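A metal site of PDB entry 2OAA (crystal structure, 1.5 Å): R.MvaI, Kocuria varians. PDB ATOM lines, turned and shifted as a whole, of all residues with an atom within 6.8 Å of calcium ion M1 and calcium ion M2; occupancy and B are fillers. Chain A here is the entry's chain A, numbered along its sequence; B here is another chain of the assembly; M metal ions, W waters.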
ATOM      1  N   GLU A  39      15.010 -15.393   8.517  1.00  0.00           N
ATOM      2  CA  GLU A  39      16.266 -15.348   9.270  1.00  0.00           C
ATOM      3  C   GLU A  39      17.178 -14.236   8.781  1.00  0.00           C
ATOM      4  O   GLU A  39      17.780 -13.532   9.597  1.00  0.00           O
ATOM      5  CB  GLU A  39      16.979 -16.723   9.275  1.00  0.00           C
ATOM      6  CG  GLU A  39      16.225 -17.797  10.101  1.00  0.00           C
ATOM      7  CD  GLU A  39      17.088 -18.979  10.592  1.00  0.00           C
ATOM      8  OE1 GLU A  39      18.154 -19.270  10.006  1.00  0.00           O
ATOM      9  OE2 GLU A  39      16.678 -19.640  11.580  1.00  0.00           O
ATOM     10  N   LYS A  44      20.197 -13.010  11.248  1.00  0.00           N
ATOM     11  CA  LYS A  44      20.654 -14.261  11.826  1.00  0.00           C
ATOM     12  C   LYS A  44      21.290 -15.096  10.726  1.00  0.00           C
ATOM     13  O   LYS A  44      20.629 -15.408   9.714  1.00  0.00           O
ATOM     14  CB  LYS A  44      19.497 -15.029  12.481  1.00  0.00           C
ATOM     15  CG  LYS A  44      19.929 -16.309  13.180  1.00  0.00           C
ATOM     16  CD  LYS A  44      18.761 -17.262  13.399  1.00  0.00           C
ATOM     17  CE  LYS A  44      19.229 -18.616  13.943  1.00  0.00           C
ATOM     18  NZ  LYS A  44      19.986 -19.386  12.905  1.00  0.00           N
ATOM     19  N   ASP A  47      22.385 -21.707  10.584  1.00  0.00           N
ATOM     20  CA  ASP A  47      23.210 -22.617  11.376  1.00  0.00           C
ATOM     21  C   ASP A  47      22.551 -23.968  11.486  1.00  0.00           C
ATOM     22  O   ASP A  47      21.395 -24.128  11.102  1.00  0.00           O
ATOM     23  CB  ASP A  47      23.506 -22.029  12.757  1.00  0.00           C
ATOM     24  CG  ASP A  47      22.319 -22.068  13.685  1.00  0.00           C
ATOM     25  OD1 ASP A  47      21.902 -23.180  14.089  1.00  0.00           O
ATOM     26  OD2 ASP A  47      21.796 -20.981  14.021  1.00  0.00           O
ATOM     27  N   ASN A  48      23.298 -24.930  12.002  1.00  0.00           N
ATOM     28  CA  ASN A  48      22.754 -26.269  12.157  1.00  0.00           C
ATOM     29  C   ASN A  48      22.738 -26.759  13.594  1.00  0.00           C
ATOM     30  O   ASN A  48      22.752 -27.966  13.855  1.00  0.00           O
ATOM     31  CB  ASN A  48      23.468 -27.253  11.212  1.00  0.00           C
ATOM     32  CG  ASN A  48      24.956 -27.338  11.464  1.00  0.00           C
ATOM     33  OD1 ASN A  48      25.446 -26.900  12.514  1.00  0.00           O
ATOM     34  ND2 ASN A  48      25.689 -27.918  10.515  1.00  0.00           N
ATOM     35  N   LEU A  49      22.712 -25.813  14.528  1.00  0.00           N
ATOM     36  CA  LEU A  49      22.655 -26.159  15.954  1.00  0.00           C
ATOM     37  C   LEU A  49      21.230 -26.424  16.413  1.00  0.00           C
ATOM     38  O   LEU A  49      20.302 -25.715  16.018  1.00  0.00           O
ATOM     39  CB  LEU A  49      23.254 -25.045  16.819  1.00  0.00           C
ATOM     40  CG  LEU A  49      24.722 -24.626  16.610  1.00  0.00           C
ATOM     41  CD1 LEU A  49      25.209 -23.933  17.884  1.00  0.00           C
ATOM     42  CD2 LEU A  49      25.636 -25.798  16.273  1.00  0.00           C
ATOM     43  N   ASP A  50      21.064 -27.444  17.256  1.00  0.00           N
ATOM     44  CA  ASP A  50      19.759 -27.723  17.877  1.00  0.00           C
ATOM     45  C   ASP A  50      19.544 -26.885  19.135  1.00  0.00           C
ATOM     46  O   ASP A  50      19.359 -27.404  20.235  1.00  0.00           O
ATOM     47  CB  ASP A  50      19.606 -29.225  18.157  1.00  0.00           C
ATOM     48  CG  ASP A  50      20.747 -29.798  19.007  1.00  0.00           C
ATOM     49  OD1 ASP A  50      21.720 -29.069  19.330  1.00  0.00           O
ATOM     50  OD2 ASP A  50      20.664 -31.000  19.351  1.00  0.00           O
ATOM     51  N   ALA A  51      19.612 -25.569  18.951  1.00  0.00           N
ATOM     52  CA  ALA A  51      19.420 -24.580  20.012  1.00  0.00           C
ATOM     53  C   ALA A  51      18.331 -23.631  19.505  1.00  0.00           C
ATOM     54  O   ALA A  51      18.038 -23.637  18.306  1.00  0.00           O
ATOM     55  CB  ALA A  51      20.711 -23.815  20.215  1.00  0.00           C
ATOM     56  N   PRO A  52      17.743 -22.810  20.402  1.00  0.00           N
ATOM     57  CA  PRO A  52      16.721 -21.891  19.898  1.00  0.00           C
ATOM     58  C   PRO A  52      17.302 -20.776  19.021  1.00  0.00           C
ATOM     59  O   PRO A  52      18.511 -20.559  19.008  1.00  0.00           O
ATOM     60  CB  PRO A  52      16.101 -21.296  21.178  1.00  0.00           C
ATOM     61  CG  PRO A  52      16.588 -22.184  22.282  1.00  0.00           C
ATOM     62  CD  PRO A  52      17.921 -22.682  21.857  1.00  0.00           C
ATOM     63  N   ASP A  53      16.424 -20.091  18.297  1.00  0.00           N
ATOM     64  CA  ASP A  53      16.849 -19.112  17.290  1.00  0.00           C
ATOM     65  C   ASP A  53      17.167 -17.744  17.855  1.00  0.00           C
ATOM     66  O   ASP A  53      18.065 -17.053  17.354  1.00  0.00           O
ATOM     67  CB  ASP A  53      15.751 -18.938  16.251  1.00  0.00           C
ATOM     68  CG  ASP A  53      15.495 -20.206  15.502  1.00  0.00           C
ATOM     69  OD1 ASP A  53      16.447 -20.737  14.883  1.00  0.00           O
ATOM     70  OD2 ASP A  53      14.346 -20.668  15.537  1.00  0.00           O
ATOM     71  N   ILE A  57      14.168 -18.560  22.631  1.00  0.00           N
ATOM     72  CA  ILE A  57      12.916 -18.726  21.879  1.00  0.00           C
ATOM     73  C   ILE A  57      13.176 -19.292  20.485  1.00  0.00           C
ATOM     74  O   ILE A  57      14.041 -18.798  19.755  1.00  0.00           O
ATOM     75  CB  ILE A  57      12.151 -17.387  21.770  1.00  0.00           C
ATOM     76  CG1 ILE A  57      11.869 -16.825  23.164  1.00  0.00           C
ATOM     77  CG2 ILE A  57      10.850 -17.570  20.976  1.00  0.00           C
ATOM     78  CD1 ILE A  57      11.647 -15.314  23.182  1.00  0.00           C
ATOM     79  N   GLU A  58      12.421 -20.328  20.119  1.00  0.00           N
ATOM     80  CA  GLU A  58      12.461 -20.910  18.795  1.00  0.00           C
ATOM     81  C   GLU A  58      11.504 -20.126  17.882  1.00  0.00           C
ATOM     82  O   GLU A  58      10.407 -19.774  18.292  1.00  0.00           O
ATOM     83  CB  GLU A  58      12.012 -22.371  18.882  1.00  0.00           C
ATOM     84  CG  GLU A  58      11.764 -23.058  17.559  1.00  0.00           C
ATOM     85  CD  GLU A  58      13.028 -23.319  16.771  1.00  0.00           C
ATOM     86  OE1 GLU A  58      14.143 -23.231  17.341  1.00  0.00           O
ATOM     87  OE2 GLU A  58      12.889 -23.634  15.556  1.00  0.00           O
ATOM     88  N   ILE A  59      11.927 -19.867  16.659  1.00  0.00           N
ATOM     89  CA  ILE A  59      11.096 -19.187  15.678  1.00  0.00           C
ATOM     90  C   ILE A  59      10.807 -20.141  14.525  1.00  0.00           C
ATOM     91  O   ILE A  59      11.691 -20.860  14.068  1.00  0.00           O
ATOM     92  CB  ILE A  59      11.813 -17.935  15.144  1.00  0.00           C
ATOM     93  CG1 ILE A  59      11.970 -16.921  16.269  1.00  0.00           C
ATOM     94  CG2 ILE A  59      11.028 -17.362  13.975  1.00  0.00           C
ATOM     95  CD1 ILE A  59      12.816 -15.718  15.889  1.00  0.00           C
ATOM     96  N   LYS A  60       9.564 -20.195  14.069  1.00  0.00           N
ATOM     97  CA  LYS A  60       9.238 -21.002  12.889  1.00  0.00           C
ATOM     98  C   LYS A  60       8.315 -20.195  12.009  1.00  0.00           C
ATOM     99  O   LYS A  60       7.366 -19.582  12.511  1.00  0.00           O
ATOM    100  CB  LYS A  60       8.533 -22.300  13.288  1.00  0.00           C
ATOM    101  CG  LYS A  60       9.333 -23.169  14.260  1.00  0.00           C
ATOM    102  CD  LYS A  60       8.719 -24.529  14.453  1.00  0.00           C
ATOM    103  CE  LYS A  60       9.593 -25.338  15.400  1.00  0.00           C
ATOM    104  NZ  LYS A  60      10.943 -25.691  14.843  1.00  0.00           N
ATOM    105  N   THR A  61       8.573 -20.186  10.707  1.00  0.00           N
ATOM    106  CA  THR A  61       7.639 -19.579   9.759  1.00  0.00           C
ATOM    107  C   THR A  61       6.750 -20.646   9.114  1.00  0.00           C
ATOM    108  O   THR A  61       7.145 -21.811   8.989  1.00  0.00           O
ATOM    109  CB  THR A  61       8.370 -18.784   8.669  1.00  0.00           C
ATOM    110  OG1 THR A  61       9.146 -19.674   7.855  1.00  0.00           O
ATOM    111  CG2 THR A  61       9.292 -17.756   9.285  1.00  0.00           C
ATOM    112  N   LYS A 162      15.510 -26.864  22.652  1.00  0.00           N
ATOM    113  CA  LYS A 162      15.102 -26.094  21.471  1.00  0.00           C
ATOM    114  C   LYS A 162      13.712 -25.471  21.578  1.00  0.00           C
ATOM    115  O   LYS A 162      13.476 -24.372  21.054  1.00  0.00           O
ATOM    116  CB  LYS A 162      15.172 -27.016  20.220  1.00  0.00           C
ATOM    117  CG  LYS A 162      14.960 -26.332  18.876  1.00  0.00           C
ATOM    118  CD  LYS A 162      14.676 -27.404  17.806  1.00  0.00           C
ATOM    119  CE  LYS A 162      14.382 -26.816  16.438  1.00  0.00           C
ATOM    120  NZ  LYS A 162      15.624 -26.599  15.658  1.00  0.00           N
ATOM    121  P    DC B   6      17.588 -29.485  14.404  1.00  0.00           P
ATOM    122  OP1  DC B   6      17.183 -28.844  15.684  1.00  0.00           O
ATOM    123  OP2  DC B   6      16.687 -30.476  13.760  1.00  0.00           O
ATOM    124  O5'  DC B   6      17.912 -28.359  13.347  1.00  0.00           O
ATOM    125  C5'  DC B   6      18.816 -27.305  13.657  1.00  0.00           C
ATOM    126  C4'  DC B   6      19.021 -26.417  12.450  1.00  0.00           C
ATOM    127  O4'  DC B   6      19.668 -27.145  11.384  1.00  0.00           O
ATOM    128  C3'  DC B   6      17.741 -25.913  11.811  1.00  0.00           C
ATOM    129  O3'  DC B   6      17.175 -24.848  12.570  1.00  0.00           O
ATOM    130  C2'  DC B   6      18.250 -25.468  10.467  1.00  0.00           C
ATOM    131  C1'  DC B   6      19.228 -26.602  10.133  1.00  0.00           C
ATOM    132  N1   DC B   6      18.619 -27.682   9.350  1.00  0.00           N
ATOM    133  C2   DC B   6      18.343 -27.438   8.001  1.00  0.00           C
ATOM    134  O2   DC B   6      18.584 -26.311   7.538  1.00  0.00           O
ATOM    135  N3   DC B   6      17.823 -28.436   7.235  1.00  0.00           N
ATOM    136  C4   DC B   6      17.575 -29.628   7.783  1.00  0.00           C
ATOM    137  N4   DC B   6      17.093 -30.579   6.978  1.00  0.00           N
ATOM    138  C5   DC B   6      17.818 -29.890   9.155  1.00  0.00           C
ATOM    139  C6   DC B   6      18.340 -28.901   9.900  1.00  0.00           C
ATOM    140  P    DT B   7      15.590 -24.616  12.541  1.00  0.00           P
ATOM    141  OP1  DT B   7      15.373 -23.378  13.348  1.00  0.00           O
ATOM    142  OP2  DT B   7      14.908 -25.874  12.946  1.00  0.00           O
ATOM    143  O5'  DT B   7      15.266 -24.313  11.024  1.00  0.00           O
ATOM    144  C5'  DT B   7      15.698 -23.094  10.426  1.00  0.00           C
ATOM    145  C4'  DT B   7      15.365 -23.064   8.949  1.00  0.00           C
ATOM    146  O4'  DT B   7      16.027 -24.133   8.238  1.00  0.00           O
ATOM    147  C3'  DT B   7      13.904 -23.281   8.606  1.00  0.00           C
ATOM    148  O3'  DT B   7      13.135 -22.119   8.927  1.00  0.00           O
ATOM    149  C2'  DT B   7      14.011 -23.550   7.126  1.00  0.00           C
ATOM    150  C1'  DT B   7      15.238 -24.473   7.098  1.00  0.00           C
ATOM    151  N1   DT B   7      14.863 -25.897   7.184  1.00  0.00           N
ATOM    152  C2   DT B   7      14.513 -26.526   6.013  1.00  0.00           C
ATOM    153  O2   DT B   7      14.529 -25.958   4.929  1.00  0.00           O
ATOM    154  N3   DT B   7      14.122 -27.831   6.149  1.00  0.00           N
ATOM    155  C4   DT B   7      14.058 -28.563   7.315  1.00  0.00           C
ATOM    156  O4   DT B   7      13.669 -29.730   7.282  1.00  0.00           O
ATOM    157  C5   DT B   7      14.461 -27.853   8.518  1.00  0.00           C
ATOM    158  C7   DT B   7      14.413 -28.560   9.832  1.00  0.00           C
ATOM    159  C6   DT B   7      14.843 -26.571   8.385  1.00  0.00           C
ATOM    160  P    DG B   8      11.549 -22.263   9.133  1.00  0.00           P
ATOM    161  OP1  DG B   8      11.020 -20.921   9.420  1.00  0.00           O
ATOM    162  OP2  DG B   8      11.284 -23.386  10.069  1.00  0.00           O
ATOM    163  O5'  DG B   8      11.076 -22.689   7.676  1.00  0.00           O
ATOM    164  C5'  DG B   8       9.894 -23.430   7.476  1.00  0.00           C
ATOM    165  C4'  DG B   8       9.911 -24.020   6.094  1.00  0.00           C
ATOM    166  O4'  DG B   8      10.841 -25.119   5.988  1.00  0.00           O
ATOM    167  C3'  DG B   8       8.607 -24.625   5.631  1.00  0.00           C
ATOM    168  O3'  DG B   8       7.702 -23.550   5.346  1.00  0.00           O
ATOM    169  C2'  DG B   8       9.090 -25.372   4.401  1.00  0.00           C
ATOM    170  C1'  DG B   8      10.424 -25.948   4.902  1.00  0.00           C
ATOM    171  N9   DG B   8      10.292 -27.314   5.376  1.00  0.00           N
ATOM    172  C8   DG B   8      10.359 -27.781   6.674  1.00  0.00           C
ATOM    173  N7   DG B   8      10.141 -29.072   6.759  1.00  0.00           N
ATOM    174  C5   DG B   8       9.923 -29.467   5.450  1.00  0.00           C
ATOM    175  C6   DG B   8       9.631 -30.754   4.903  1.00  0.00           C
ATOM    176  O6   DG B   8       9.489 -31.832   5.480  1.00  0.00           O
ATOM    177  N1   DG B   8       9.506 -30.698   3.511  1.00  0.00           N
ATOM    178  C2   DG B   8       9.648 -29.569   2.750  1.00  0.00           C
ATOM    179  N2   DG B   8       9.493 -29.721   1.431  1.00  0.00           N
ATOM    180  N3   DG B   8       9.901 -28.367   3.249  1.00  0.00           N
ATOM    181  C4   DG B   8      10.037 -28.399   4.589  1.00  0.00           C
HETATM  182 CA    CA M   1      13.601 -22.072  13.842  1.00  0.00          CA
HETATM  183 CA    CA M   2      17.539 -22.721  14.392  1.00  0.00          CA
HETATM  184  O   HOH W   1      14.233 -20.438  12.253  1.00  0.00           O
HETATM  185  O   HOH W   2      19.718 -23.643  14.314  1.00  0.00           O
HETATM  186  O   HOH W   3      12.460 -23.552  12.414  1.00  0.00           O
HETATM  187  O   HOH W   4      19.029 -21.604  16.091  1.00  0.00           O
HETATM  188  O   HOH W   5      18.507 -21.768  12.516  1.00  0.00           O
HETATM  189  O   HOH W   6      16.416 -23.839  16.271  1.00  0.00           O
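OP2 of DT 7 of chain B lies within salt-bridge range of NZ of Lys 162 (2.9 Å). The side-chain carboxylate (OE2) of Glu 58 sits close to the side-chain amino group (NZ) of Lys 60, 2.9 Å away. OP1 of DC 6 of chain B lies within salt-bridge range of NZ of Lys 162 (2.7 Å).
Of the 18 residues printed, 4 come within 4 Å of calcium ion M1. The nearest printed residue that does not touch calcium ion M1 is Lys 60 (4.4 Å).
Within 4 Å of calcium ion M2: Asp 53, DC 6 of chain B and DT 7 of chain B. The nearest printed residue that does not touch calcium ion M2 is Ala 51 (4.1 Å).
Calcium ion M1 is bound by OP1 of DT 7 of chain B, the backbone carbonyl oxygen (O) of Ile 59, the side-chain carboxylate (OD2) of Asp 53, water W3, water W1 and the side-chain carboxylate (OE2) of Glu 58.
Calcium ion M2 is bound by water W5 (2.3 Å), the side-chain carboxylate (OD1) of Asp 53 (2.3 Å), water W2 (2.4 Å), water W6 (2.5 Å), OP1 of DT 7 of chain B (2.5 Å), water W4 (2.5 Å) and O3' of DC 6 of chain B (2.8 Å). Calcium ion M2 has seven donor atoms within binding distance.
Water W2 bridges O of Leu 49 and OD2 of Asp 47. Water W6 lies within hydrogen-bond range of OE1 of Glu 58, O of Ala 51 and NZ of Lys 162. Water W5 bridges NZ of Lys 44 and OE2 of Glu 39.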
